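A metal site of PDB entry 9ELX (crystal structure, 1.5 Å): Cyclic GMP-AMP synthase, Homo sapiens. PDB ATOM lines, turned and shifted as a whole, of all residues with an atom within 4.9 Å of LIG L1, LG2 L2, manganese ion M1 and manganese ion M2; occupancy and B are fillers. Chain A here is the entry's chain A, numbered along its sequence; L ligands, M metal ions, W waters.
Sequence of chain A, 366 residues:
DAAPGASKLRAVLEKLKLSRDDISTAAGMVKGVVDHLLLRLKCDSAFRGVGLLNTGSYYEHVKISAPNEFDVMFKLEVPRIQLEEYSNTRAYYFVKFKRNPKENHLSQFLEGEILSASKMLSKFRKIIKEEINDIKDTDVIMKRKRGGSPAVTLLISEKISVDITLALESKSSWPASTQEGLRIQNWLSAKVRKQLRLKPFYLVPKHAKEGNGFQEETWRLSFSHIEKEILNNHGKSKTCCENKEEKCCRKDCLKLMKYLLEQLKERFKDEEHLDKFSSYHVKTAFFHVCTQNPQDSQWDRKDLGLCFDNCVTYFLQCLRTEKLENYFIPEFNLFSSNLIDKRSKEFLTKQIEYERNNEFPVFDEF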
ATOM      1  N   THR A  55     -15.594  29.231 -24.904  1.00  0.00           N
ATOM      2  CA  THR A  55     -16.800  28.575 -24.363  1.00  0.00           C
ATOM      3  C   THR A  55     -16.435  27.801 -23.121  1.00  0.00           C
ATOM      4  O   THR A  55     -15.282  27.694 -22.703  1.00  0.00           O
ATOM      5  CB  THR A  55     -17.426  27.587 -25.376  1.00  0.00           C
ATOM      6  OG1 THR A  55     -16.491  26.532 -25.629  1.00  0.00           O
ATOM      7  CG2 THR A  55     -17.721  28.284 -26.703  1.00  0.00           C
ATOM      8  N   GLY A  56     -17.448  27.257 -22.467  1.00  0.00           N
ATOM      9  CA  GLY A  56     -17.149  26.346 -21.357  1.00  0.00           C
ATOM     10  C   GLY A  56     -16.827  27.023 -20.035  1.00  0.00           C
ATOM     11  O   GLY A  56     -16.853  28.258 -19.925  1.00  0.00           O
ATOM     12  N   SER A  57     -16.460  26.205 -19.030  1.00  0.00           N
ATOM     13  CA  SER A  57     -16.520  26.700 -17.660  1.00  0.00           C
ATOM     14  C   SER A  57     -15.490  27.780 -17.359  1.00  0.00           C
ATOM     15  O   SER A  57     -15.729  28.631 -16.492  1.00  0.00           O
ATOM     16  CB  SER A  57     -16.371  25.562 -16.691  1.00  0.00           C
ATOM     17  OG  SER A  57     -15.075  24.942 -16.808  1.00  0.00           O
ATOM     18  N   GLU A  60     -16.996  30.966 -18.434  1.00  0.00           N
ATOM     19  CA  GLU A  60     -18.152  31.299 -17.605  1.00  0.00           C
ATOM     20  C   GLU A  60     -17.807  31.508 -16.150  1.00  0.00           C
ATOM     21  O   GLU A  60     -18.701  31.699 -15.319  1.00  0.00           O
ATOM     22  CB  GLU A  60     -19.243  30.192 -17.745  1.00  0.00           C
ATOM     23  CG  GLU A  60     -19.319  29.724 -19.199  1.00  0.00           C
ATOM     24  CD  GLU A  60     -20.107  28.376 -19.422  1.00  0.00           C
ATOM     25  OE1 GLU A  60     -20.986  28.283 -20.331  1.00  0.00           O
ATOM     26  OE2 GLU A  60     -19.893  27.449 -18.589  1.00  0.00           O
ATOM     27  N   LYS A  63     -15.218  27.345 -13.713  1.00  0.00           N
ATOM     28  CA  LYS A  63     -14.186  26.315 -13.608  1.00  0.00           C
ATOM     29  C   LYS A  63     -13.729  26.208 -12.152  1.00  0.00           C
ATOM     30  O   LYS A  63     -13.522  27.243 -11.469  1.00  0.00           O
ATOM     31  CB  LYS A  63     -13.005  26.745 -14.509  1.00  0.00           C
ATOM     32  CG  LYS A  63     -11.804  25.734 -14.483  1.00  0.00           C
ATOM     33  CD  LYS A  63     -12.107  24.558 -15.409  1.00  0.00           C
ATOM     34  CE  LYS A  63     -11.077  23.422 -15.277  1.00  0.00           C
ATOM     35  NZ  LYS A  63     -11.200  22.705 -13.958  1.00  0.00           N
ATOM     36  N   GLU A  69      -8.323  23.212 -17.989  1.00  0.00           N
ATOM     37  CA  GLU A  69      -9.172  22.683 -19.059  1.00  0.00           C
ATOM     38  C   GLU A  69      -9.979  23.820 -19.651  1.00  0.00           C
ATOM     39  O   GLU A  69     -10.767  24.504 -18.962  1.00  0.00           O
ATOM     40  CB  GLU A  69     -10.077  21.562 -18.535  1.00  0.00           C
ATOM     41  CG  GLU A  69     -10.528  20.574 -19.679  1.00  0.00           C
ATOM     42  CD  GLU A  69     -11.881  20.923 -20.285  1.00  0.00           C
ATOM     43  OE1 GLU A  69     -12.409  22.018 -19.963  1.00  0.00           O
ATOM     44  OE2 GLU A  69     -12.406  20.096 -21.075  1.00  0.00           O
ATOM     45  N   PHE A  70      -9.700  24.080 -20.942  1.00  0.00           N
ATOM     46  CA  PHE A  70     -10.267  25.198 -21.668  1.00  0.00           C
ATOM     47  C   PHE A  70     -11.019  24.672 -22.871  1.00  0.00           C
ATOM     48  O   PHE A  70     -10.588  23.712 -23.483  1.00  0.00           O
ATOM     49  CB  PHE A  70      -9.183  26.157 -22.148  1.00  0.00           C
ATOM     50  CG  PHE A  70      -8.473  26.894 -21.051  1.00  0.00           C
ATOM     51  CD1 PHE A  70      -7.541  26.237 -20.254  1.00  0.00           C
ATOM     52  CD2 PHE A  70      -8.680  28.261 -20.876  1.00  0.00           C
ATOM     53  CE1 PHE A  70      -6.859  26.918 -19.288  1.00  0.00           C
ATOM     54  CE2 PHE A  70      -7.948  28.969 -19.899  1.00  0.00           C
ATOM     55  CZ  PHE A  70      -7.073  28.274 -19.082  1.00  0.00           C
ATOM     56  N   ASP A  71     -12.076  25.385 -23.255  1.00  0.00           N
ATOM     57  CA  ASP A  71     -12.894  24.999 -24.385  1.00  0.00           C
ATOM     58  C   ASP A  71     -13.031  26.163 -25.339  1.00  0.00           C
ATOM     59  O   ASP A  71     -13.235  27.288 -24.897  1.00  0.00           O
ATOM     60  CB  ASP A  71     -14.279  24.560 -23.923  1.00  0.00           C
ATOM     61  CG  ASP A  71     -14.188  23.468 -22.917  1.00  0.00           C
ATOM     62  OD1 ASP A  71     -13.815  22.326 -23.261  1.00  0.00           O
ATOM     63  OD2 ASP A  71     -14.446  23.754 -21.722  1.00  0.00           O
ATOM     64  N   ARG A 146     -11.294  10.993 -28.599  1.00  0.00           N
ATOM     65  CA  ARG A 146     -12.235  10.375 -27.680  1.00  0.00           C
ATOM     66  C   ARG A 146     -13.574  10.195 -28.405  1.00  0.00           C
ATOM     67  O   ARG A 146     -14.074  11.129 -29.037  1.00  0.00           O
ATOM     68  CB  ARG A 146     -12.390  11.164 -26.367  1.00  0.00           C
ATOM     69  CG  ARG A 146     -13.333  12.347 -26.354  1.00  0.00           C
ATOM     70  CD  ARG A 146     -13.636  12.900 -24.941  1.00  0.00           C
ATOM     71  NE  ARG A 146     -12.592  13.708 -24.292  1.00  0.00           N
ATOM     72  CZ  ARG A 146     -12.367  14.999 -24.512  1.00  0.00           C
ATOM     73  NH1 ARG A 146     -13.045  15.682 -25.417  1.00  0.00           N
ATOM     74  NH2 ARG A 146     -11.444  15.637 -23.776  1.00  0.00           N
ATOM     75  N   GLY A 148     -17.241   9.849 -29.845  1.00  0.00           N
ATOM     76  CA  GLY A 148     -18.408  10.688 -29.671  1.00  0.00           C
ATOM     77  C   GLY A 148     -18.107  12.163 -29.473  1.00  0.00           C
ATOM     78  O   GLY A 148     -19.043  12.959 -29.382  1.00  0.00           O
ATOM     79  N   SER A 149     -16.830  12.548 -29.389  1.00  0.00           N
ATOM     80  CA  SER A 149     -16.628  13.975 -29.134  1.00  0.00           C
ATOM     81  C   SER A 149     -16.479  14.745 -30.422  1.00  0.00           C
ATOM     82  O   SER A 149     -15.818  14.276 -31.353  1.00  0.00           O
ATOM     83  CB  SER A 149     -15.379  14.214 -28.298  1.00  0.00           C
ATOM     84  OG  SER A 149     -15.180  15.600 -28.043  1.00  0.00           O
ATOM     85  N   PRO A 150     -17.005  15.967 -30.511  1.00  0.00           N
ATOM     86  CA  PRO A 150     -16.734  16.795 -31.672  1.00  0.00           C
ATOM     87  C   PRO A 150     -15.438  17.570 -31.545  1.00  0.00           C
ATOM     88  O   PRO A 150     -15.115  18.280 -32.479  1.00  0.00           O
ATOM     89  CB  PRO A 150     -17.928  17.753 -31.703  1.00  0.00           C
ATOM     90  CG  PRO A 150     -18.202  18.001 -30.250  1.00  0.00           C
ATOM     91  CD  PRO A 150     -17.896  16.650 -29.551  1.00  0.00           C
ATOM     92  N   ALA A 151     -14.748  17.469 -30.391  1.00  0.00           N
ATOM     93  CA  ALA A 151     -13.568  18.291 -30.153  1.00  0.00           C
ATOM     94  C   ALA A 151     -12.310  17.573 -30.610  1.00  0.00           C
ATOM     95  O   ALA A 151     -12.236  16.328 -30.632  1.00  0.00           O
ATOM     96  CB  ALA A 151     -13.454  18.628 -28.654  1.00  0.00           C
ATOM     97  N   ASP A 163      -9.899  21.848 -25.544  1.00  0.00           N
ATOM     98  CA  ASP A 163     -10.796  21.198 -26.497  1.00  0.00           C
ATOM     99  C   ASP A 163     -11.145  22.214 -27.548  1.00  0.00           C
ATOM    100  O   ASP A 163     -11.719  23.260 -27.211  1.00  0.00           O
ATOM    101  CB  ASP A 163     -12.080  20.712 -25.813  1.00  0.00           C
ATOM    102  CG  ASP A 163     -11.836  19.573 -24.923  1.00  0.00           C
ATOM    103  OD1 ASP A 163     -11.340  18.514 -25.326  1.00  0.00           O
ATOM    104  OD2 ASP A 163     -12.329  19.598 -23.785  1.00  0.00           O
ATOM    105  N   THR A 165     -13.349  22.824 -30.843  1.00  0.00           N
ATOM    106  CA  THR A 165     -14.468  22.233 -31.569  1.00  0.00           C
ATOM    107  C   THR A 165     -14.713  23.025 -32.836  1.00  0.00           C
ATOM    108  O   THR A 165     -14.975  24.231 -32.785  1.00  0.00           O
ATOM    109  CB  THR A 165     -15.722  22.194 -30.699  1.00  0.00           C
ATOM    110  OG1 THR A 165     -15.503  21.327 -29.582  1.00  0.00           O
ATOM    111  CG2 THR A 165     -16.957  21.695 -31.481  1.00  0.00           C
ATOM    112  N   VAL A 204     -21.934  21.446 -34.731  1.00  0.00           N
ATOM    113  CA  VAL A 204     -20.636  20.855 -34.432  1.00  0.00           C
ATOM    114  C   VAL A 204     -20.667  19.393 -34.884  1.00  0.00           C
ATOM    115  O   VAL A 204     -21.748  18.772 -34.990  1.00  0.00           O
ATOM    116  CB  VAL A 204     -20.274  21.004 -32.934  1.00  0.00           C
ATOM    117  CG1 VAL A 204     -20.257  22.475 -32.544  1.00  0.00           C
ATOM    118  CG2 VAL A 204     -21.307  20.230 -32.080  1.00  0.00           C
ATOM    119  N   LYS A 206     -20.647  16.371 -33.960  1.00  0.00           N
ATOM    120  CA  LYS A 206     -21.061  15.283 -33.079  1.00  0.00           C
ATOM    121  C   LYS A 206     -22.206  14.583 -33.779  1.00  0.00           C
ATOM    122  O   LYS A 206     -23.203  15.225 -34.144  1.00  0.00           O
ATOM    123  CB  LYS A 206     -21.483  15.834 -31.708  1.00  0.00           C
ATOM    124  CG  LYS A 206     -21.840  14.731 -30.713  1.00  0.00           C
ATOM    125  CD  LYS A 206     -22.412  15.336 -29.454  1.00  0.00           C
ATOM    126  CE  LYS A 206     -22.761  14.277 -28.392  1.00  0.00           C
ATOM    127  NZ  LYS A 206     -21.626  13.399 -28.074  1.00  0.00           N
ATOM    128  N   ARG A 220     -24.505  18.364 -34.874  1.00  0.00           N
ATOM    129  CA  ARG A 220     -25.286  18.586 -33.665  1.00  0.00           C
ATOM    130  C   ARG A 220     -25.443  20.080 -33.431  1.00  0.00           C
ATOM    131  O   ARG A 220     -24.483  20.837 -33.538  1.00  0.00           O
ATOM    132  CB  ARG A 220     -24.599  17.928 -32.462  1.00  0.00           C
ATOM    133  CG  ARG A 220     -25.051  18.513 -31.150  1.00  0.00           C
ATOM    134  CD  ARG A 220     -26.401  17.964 -30.743  1.00  0.00           C
ATOM    135  NE  ARG A 220     -26.186  16.779 -29.951  1.00  0.00           N
ATOM    136  CZ  ARG A 220     -26.123  16.769 -28.620  1.00  0.00           C
ATOM    137  NH1 ARG A 220     -26.194  17.886 -27.922  1.00  0.00           N
ATOM    138  NH2 ARG A 220     -25.925  15.603 -28.000  1.00  0.00           N
ATOM    139  N   LEU A 221     -26.662  20.514 -33.117  1.00  0.00           N
ATOM    140  CA  LEU A 221     -26.894  21.905 -32.745  1.00  0.00           C
ATOM    141  C   LEU A 221     -26.158  22.252 -31.464  1.00  0.00           C
ATOM    142  O   LEU A 221     -26.154  21.462 -30.501  1.00  0.00           O
ATOM    143  CB  LEU A 221     -28.383  22.132 -32.496  1.00  0.00           C
ATOM    144  CG  LEU A 221     -29.297  22.207 -33.681  1.00  0.00           C
ATOM    145  CD1 LEU A 221     -30.695  22.507 -33.100  1.00  0.00           C
ATOM    146  CD2 LEU A 221     -28.833  23.319 -34.652  1.00  0.00           C
ATOM    147  N   SER A 222     -25.573  23.434 -31.421  1.00  0.00           N
ATOM    148  CA  SER A 222     -24.866  23.893 -30.245  1.00  0.00           C
ATOM    149  C   SER A 222     -25.190  25.341 -29.983  1.00  0.00           C
ATOM    150  O   SER A 222     -25.122  26.208 -30.874  1.00  0.00           O
ATOM    151  CB  SER A 222     -23.340  23.739 -30.372  1.00  0.00           C
ATOM    152  OG  SER A 222     -22.726  24.277 -29.188  1.00  0.00           O
ATOM    153  N   SER A 224     -23.538  26.793 -27.107  1.00  0.00           N
ATOM    154  CA  SER A 224     -22.569  27.035 -26.034  1.00  0.00           C
ATOM    155  C   SER A 224     -22.387  28.543 -25.803  1.00  0.00           C
ATOM    156  O   SER A 224     -22.201  28.982 -24.660  1.00  0.00           O
ATOM    157  CB  SER A 224     -21.203  26.413 -26.382  1.00  0.00           C
ATOM    158  OG  SER A 224     -21.235  25.003 -26.443  1.00  0.00           O
ATOM    159  N   GLU A 227     -25.174  29.756 -23.586  1.00  0.00           N
ATOM    160  CA  GLU A 227     -24.911  29.335 -22.188  1.00  0.00           C
ATOM    161  C   GLU A 227     -23.929  30.272 -21.486  1.00  0.00           C
ATOM    162  O   GLU A 227     -24.113  30.621 -20.305  1.00  0.00           O
ATOM    163  CB  GLU A 227     -24.428  27.875 -22.105  1.00  0.00           C
ATOM    164  CG  GLU A 227     -25.410  26.939 -22.830  1.00  0.00           C
ATOM    165  CD  GLU A 227     -24.903  25.498 -22.935  1.00  0.00           C
ATOM    166  OE1 GLU A 227     -23.733  25.198 -22.522  1.00  0.00           O
ATOM    167  OE2 GLU A 227     -25.657  24.675 -23.575  1.00  0.00           O
ATOM    168  N   LYS A 258     -20.966  20.828  -9.662  1.00  0.00           N
ATOM    169  CA  LYS A 258     -19.911  20.286 -10.502  1.00  0.00           C
ATOM    170  C   LYS A 258     -18.929  19.505  -9.654  1.00  0.00           C
ATOM    171  O   LYS A 258     -18.445  18.452 -10.075  1.00  0.00           O
ATOM    172  CB  LYS A 258     -19.181  21.436 -11.247  1.00  0.00           C
ATOM    173  CG  LYS A 258     -20.020  22.101 -12.364  1.00  0.00           C
ATOM    174  CD  LYS A 258     -19.341  23.444 -12.857  1.00  0.00           C
ATOM    175  CE  LYS A 258     -17.870  23.222 -13.366  1.00  0.00           C
ATOM    176  NZ  LYS A 258     -18.010  22.542 -14.684  1.00  0.00           N
ATOM    177  N   GLU A 262     -17.858  15.713  -9.977  1.00  0.00           N
ATOM    178  CA  GLU A 262     -16.441  15.443 -10.201  1.00  0.00           C
ATOM    179  C   GLU A 262     -15.919  14.459  -9.152  1.00  0.00           C
ATOM    180  O   GLU A 262     -15.230  13.482  -9.464  1.00  0.00           O
ATOM    181  CB  GLU A 262     -15.606  16.751 -10.185  1.00  0.00           C
ATOM    182  CG  GLU A 262     -15.654  17.645 -11.502  1.00  0.00           C
ATOM    183  CD  GLU A 262     -14.652  18.836 -11.559  1.00  0.00           C
ATOM    184  OE1 GLU A 262     -13.605  18.752 -10.894  1.00  0.00           O
ATOM    185  OE2 GLU A 262     -14.885  19.856 -12.307  1.00  0.00           O
ATOM    186  N   SER A 279     -20.392  16.772 -16.605  1.00  0.00           N
ATOM    187  CA  SER A 279     -20.702  18.089 -16.067  1.00  0.00           C
ATOM    188  C   SER A 279     -21.792  18.791 -16.838  1.00  0.00           C
ATOM    189  O   SER A 279     -22.477  19.640 -16.255  1.00  0.00           O
ATOM    190  CB  SER A 279     -19.439  18.996 -16.049  1.00  0.00           C
ATOM    191  OG  SER A 279     -19.049  19.351 -17.362  1.00  0.00           O
ATOM    192  N   TYR A 280     -22.009  18.445 -18.120  1.00  0.00           N
ATOM    193  CA  TYR A 280     -23.127  19.088 -18.823  1.00  0.00           C
ATOM    194  C   TYR A 280     -24.463  18.699 -18.255  1.00  0.00           C
ATOM    195  O   TYR A 280     -25.428  19.469 -18.372  1.00  0.00           O
ATOM    196  CB  TYR A 280     -23.060  18.747 -20.319  1.00  0.00           C
ATOM    197  CG  TYR A 280     -23.930  19.618 -21.144  1.00  0.00           C
ATOM    198  CD1 TYR A 280     -23.622  20.981 -21.266  1.00  0.00           C
ATOM    199  CD2 TYR A 280     -25.058  19.106 -21.769  1.00  0.00           C
ATOM    200  CE1 TYR A 280     -24.404  21.817 -21.984  1.00  0.00           C
ATOM    201  CE2 TYR A 280     -25.848  19.972 -22.570  1.00  0.00           C
ATOM    202  CZ  TYR A 280     -25.525  21.313 -22.617  1.00  0.00           C
ATOM    203  OH  TYR A 280     -26.348  22.152 -23.343  1.00  0.00           O
ATOM    204  N   LYS A 283     -24.869  21.122 -15.475  1.00  0.00           N
ATOM    205  CA  LYS A 283     -25.092  22.465 -15.984  1.00  0.00           C
ATOM    206  C   LYS A 283     -26.531  22.633 -16.487  1.00  0.00           C
ATOM    207  O   LYS A 283     -27.193  23.649 -16.231  1.00  0.00           O
ATOM    208  CB  LYS A 283     -24.085  22.722 -17.085  1.00  0.00           C
ATOM    209  CG  LYS A 283     -24.045  24.194 -17.572  1.00  0.00           C
ATOM    210  CD  LYS A 283     -23.172  24.263 -18.820  1.00  0.00           C
ATOM    211  CE  LYS A 283     -22.879  25.772 -19.153  1.00  0.00           C
ATOM    212  NZ  LYS A 283     -22.035  25.848 -20.382  1.00  0.00           N
HETATM  213  C1  LIG L   1     -19.242  16.142 -26.146  1.00  0.00           C
HETATM  214  N1  LIG L   1     -17.755  15.680 -24.237  1.00  0.00           N
HETATM  215  C2  LIG L   1     -16.403  15.799 -24.237  1.00  0.00           C
HETATM  216  C3  LIG L   1     -15.232  15.548 -22.086  1.00  0.00           C
HETATM  217  C4  LIG L   1     -14.152  17.427 -21.083  1.00  0.00           C
HETATM  218  C5  LIG L   1     -15.719  18.746 -24.243  1.00  0.00           C
HETATM  219  C6  LIG L   1     -20.358  20.797 -28.198  1.00  0.00           C
HETATM  220  C7  LIG L   1     -19.075  20.868 -27.733  1.00  0.00           C
HETATM  221  C8  LIG L   1     -18.640  19.750 -27.044  1.00  0.00           C
HETATM  222  C9  LIG L   1     -19.422  18.597 -26.836  1.00  0.00           C
HETATM  223  C10 LIG L   1     -20.711  18.562 -27.339  1.00  0.00           C
HETATM  224  C11 LIG L   1     -21.145  19.701 -28.039  1.00  0.00           C
HETATM  225  C12 LIG L   1     -18.515  15.106 -25.332  1.00  0.00           C
HETATM  226  C13 LIG L   1     -15.668  16.348 -23.131  1.00  0.00           C
HETATM  227  C14 LIG L   1     -14.455  16.058 -21.025  1.00  0.00           C
HETATM  228  C15 LIG L   1     -15.271  17.705 -23.125  1.00  0.00           C
HETATM  229  F1  LIG L   1     -20.848  21.891 -28.910  1.00  0.00           F
HETATM  230  N2  LIG L   1     -18.862  17.503 -26.126  1.00  0.00           N
HETATM  231  N3  LIG L   1     -14.532  18.179 -22.134  1.00  0.00           N
HETATM  232  O1  LIG L   1     -15.236  19.860 -24.154  1.00  0.00           O
HETATM  233  O2  LIG L   1     -16.568  18.342 -25.046  1.00  0.00           O
HETATM  234  O3  LIG L   1     -15.821  15.423 -25.252  1.00  0.00           O
HETATM  235  O4  LIG L   1     -20.192  15.772 -26.853  1.00  0.00           O
HETATM  236 CL1  LIG L   1     -22.743  19.726 -28.649  1.00  0.00          CL
HETATM  237  P1  LG2 L   2     -15.741  21.507 -16.921  1.00  0.00           P
HETATM  238  O1  LG2 L   2     -15.523  22.556 -15.928  1.00  0.00           O
HETATM  239  O2  LG2 L   2     -15.815  20.095 -16.267  1.00  0.00           O
HETATM  240  O3  LG2 L   2     -14.718  21.549 -18.014  1.00  0.00           O
HETATM  241  P2  LG2 L   2     -17.560  22.554 -19.007  1.00  0.00           P
HETATM  242  O4  LG2 L   2     -18.890  23.209 -18.940  1.00  0.00           O
HETATM  243  O5  LG2 L   2     -16.418  23.446 -19.512  1.00  0.00           O
HETATM  244  N1  LG2 L   2     -17.269  21.836 -17.538  1.00  0.00           N
HETATM  245  P3  LG2 L   2     -16.918  20.628 -21.161  1.00  0.00           P
HETATM  246  O6  LG2 L   2     -17.246  19.171 -21.088  1.00  0.00           O
HETATM  247  O7  LG2 L   2     -15.449  21.020 -21.091  1.00  0.00           O
HETATM  248  O8  LG2 L   2     -17.757  21.374 -20.017  1.00  0.00           O
HETATM  249  O9  LG2 L   2     -17.600  21.206 -22.435  1.00  0.00           O
HETATM  250  C1  LG2 L   2     -17.384  22.582 -22.773  1.00  0.00           C
HETATM  251  C2  LG2 L   2     -18.716  23.162 -23.206  1.00  0.00           C
HETATM  252  O10 LG2 L   2     -19.148  22.433 -24.377  1.00  0.00           O
HETATM  253  C3  LG2 L   2     -19.873  23.024 -22.244  1.00  0.00           C
HETATM  254  O11 LG2 L   2     -19.929  24.085 -21.296  1.00  0.00           O
HETATM  255  C4  LG2 L   2     -21.076  23.103 -23.174  1.00  0.00           C
HETATM  256  O12 LG2 L   2     -21.311  24.459 -23.547  1.00  0.00           O
HETATM  257  C5  LG2 L   2     -20.567  22.324 -24.375  1.00  0.00           C
HETATM  258  N2  LG2 L   2     -20.933  20.907 -24.265  1.00  0.00           N
HETATM  259  C6  LG2 L   2     -20.238  19.904 -23.631  1.00  0.00           C
HETATM  260  N3  LG2 L   2     -20.871  18.751 -23.599  1.00  0.00           N
HETATM  261  C7  LG2 L   2     -22.053  19.012 -24.267  1.00  0.00           C
HETATM  262  C8  LG2 L   2     -23.166  18.209 -24.586  1.00  0.00           C
HETATM  263  N4  LG2 L   2     -23.240  16.908 -24.276  1.00  0.00           N
HETATM  264  N5  LG2 L   2     -24.194  18.798 -25.224  1.00  0.00           N
HETATM  265  C9  LG2 L   2     -24.102  20.085 -25.558  1.00  0.00           C
HETATM  266  N6  LG2 L   2     -23.109  20.951 -25.307  1.00  0.00           N
HETATM  267  C10 LG2 L   2     -22.116  20.340 -24.660  1.00  0.00           C
HETATM  268 MN    MN M   1     -13.892  20.323 -22.533  1.00  0.00          MN
HETATM  269 MN    MN M   2     -14.464  22.586 -19.884  1.00  0.00          MN
HETATM  270  O   HOH W   1     -15.846  17.808 -17.671  1.00  0.00           O
HETATM  271  O   HOH W   2     -14.062  22.509 -13.484  1.00  0.00           O
HETATM  272  O   HOH W   3     -19.717  25.108 -17.205  1.00  0.00           O
HETATM  273  O   HOH W   4     -20.968  21.412 -18.538  1.00  0.00           O
HETATM  274  O   HOH W   5     -16.978  19.807 -13.799  1.00  0.00           O
HETATM  275  O   HOH W   6     -27.024  17.908 -24.951  1.00  0.00           O
HETATM  276  O   HOH W   7     -20.529  22.600 -15.922  1.00  0.00           O
HETATM  277  O   HOH W   8     -23.307  23.361 -26.692  1.00  0.00           O
HETATM  278  O   HOH W   9     -25.626  15.115 -25.379  1.00  0.00           O
HETATM  279  O   HOH W  10     -19.922  24.347 -28.926  1.00  0.00           O
HETATM  280  O   HOH W  11     -19.030  17.136 -22.076  1.00  0.00           O
HETATM  281  O   HOH W  12     -12.697  19.676 -17.471  1.00  0.00           O
HETATM  282  O   HOH W  13     -13.548  24.424 -18.929  1.00  0.00           O
HETATM  283  O   HOH W  14     -16.293  21.757 -25.848  1.00  0.00           O
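Residues that only touch manganese ion M2: Ser 57 (3.9 Å). Three residues have an atom within 4 Å of manganese ion M2: Ser 57, Glu 69 and Asp 71.
Manganese ion M2 is bound by the side-chain carboxylate of Glu 69 (2.1 Å), an oxygen (O3) of LG2 L2 (2.2 Å), an oxygen (O5) of LG2 L2 (2.2 Å), the side-chain carboxylate of Asp 71 (2.2 Å), an oxygen (O7) of LG2 L2 (2.2 Å) and water W13 (2.3 Å).
Within 4 Å of manganese ion M1: Glu 69, Asp 71 and Asp 163.
Manganese ion M1 is bound by the side-chain carboxylate of Glu 69 (2.1 Å), the side-chain carboxylate of Asp 163 (2.1 Å), the side-chain carboxylate of Asp 71 (2.1 Å), an oxygen (O1) of LIG L1 (2.2 Å), an oxygen (O7) of LG2 L2 (2.2 Å) and a nitrogen (N3) of LIG L1 (2.3 Å).
CA of Gly 56 touches O5 of LG2 L2, 3.5 Å away. Lys 63 touches LG2 L2 (CD to O1, 3.99 Å). Tyr 280 touches LG2 L2. Hydrophobic or aromatic side chains within 4 Å of LG2 L2: Tyr 280. Of the 27 residues printed, 12 come within 4 Å of LG2 L2. The nearest printed residue that does not touch LG2 L2 is Glu 262 (4.1 Å).
An oxygen (O1) of LG2 L2 is in salt-bridge range of the side-chain amino group (NZ) of Lys 258 (2.8 Å). The backbone NH of Ser 57 sits close to an oxygen (O5) of LG2 L2, at 2.8 Å. An oxygen (O1) of LG2 L2 lies within hydrogen-bond range of the side-chain hydroxyl of Ser 57, at 2.6 Å. An oxygen (O3) of LIG L1 lies within hydrogen-bond range of the guanidinium group (NH1) of Arg 146 (2.8 Å). The side-chain amino group (NZ) of Lys 206 lies within hydrogen-bond range of an oxygen (O4) of LIG L1. An oxygen (O12) of LG2 L2 sits at hydrogen-bond distance from the side-chain carboxylate of Glu 227 (2.7 Å). OG of Ser 279 is in hydrogen-bond range of N1 of LG2 L2. The side-chain hydroxyl (OG) of Ser 149 sits at hydrogen-bond distance from an oxygen (O3) of LIG L1. O11 of LG2 L2 lies within hydrogen-bond range of NZ of Lys 283 (2.9 Å). A nitrogen (N5) of LG2 L2 lies within hydrogen-bond range of the guanidinium group (NH1) of Arg 220, 3.5 Å away. OG of Ser 224 is in hydrogen-bond range of O12 of LG2 L2.
Water W10 lies within hydrogen-bond range of OG of Ser 222 and OG of Ser 224. Water W3 lies within hydrogen-bond range of O4 of LG2 L2 (2.7 Å) and OE2 of Glu 60 (2.7 Å). Water W8 lies within hydrogen-bond range of OG of Ser 224, OG of Ser 222 and N6 of LG2 L2. Water W2 lies within hydrogen-bond range of an oxygen (O1) of LG2 L2, the side-chain amino group (NZ) of Lys 63 and the side-chain carboxylate (OE2) of Glu 262. Water W11 lies within hydrogen-bond range of O6 of LG2 L2 (2.9 Å) and N1 of LIG L1 (2.9 Å). Water W9 lies within hydrogen-bond range of NH2 of Arg 220 (2.7 Å) and N4 of LG2 L2 (3.2 Å).
OG of Ser 222 sits close to F1 of LIG L1, at 3.0 Å. Merely in contact with LIG L1: Gly 148, Pro 150, Val 204, Arg 220 and Ser 224. Hydrophobic or aromatic side chains that line LIG L1: Pro 150 and Val 204. 12 residues have an atom within 4 Å of LIG L1: Glu 69, Asp 71, Arg 146, Gly 148, Ser 149, Pro 150, Asp 163, Val 204, Lys 206, Arg 220, Ser 222 and Ser 224. The nearest printed residue that does not touch LIG L1 is Thr 165 (4.05 Å).
The backbone carbonyl oxygen of Ser 57 is in hydrogen-bond range of the backbone NH of Lys 63 (3.1 Å). The backbone NH (N) of Arg 220 lies within hydrogen-bond range of the backbone carbonyl oxygen (O) of Val 204. N of Thr 55 lies within hydrogen-bond range of O of Asp 71, 3.1 Å away. OH of Tyr 280 lies within hydrogen-bond range of OE2 of Glu 227 (2.6 Å). The guanidinium group (NH1) of Arg 146 is in hydrogen-bond range of the side-chain hydroxyl (OG) of Ser 149 (3.4 Å). The backbone carbonyl oxygen of Phe 70 lies within hydrogen-bond range of the backbone NH of Asp 163, 2.9 Å away. The side-chain hydroxyl (OG) of Ser 149 is in hydrogen-bond range of the backbone NH (N) of Ala 151. The side-chain carboxylate (OD1) of Asp 163 lies within salt-bridge range of the guanidinium group (NH2) of Arg 146 (3.3 Å).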
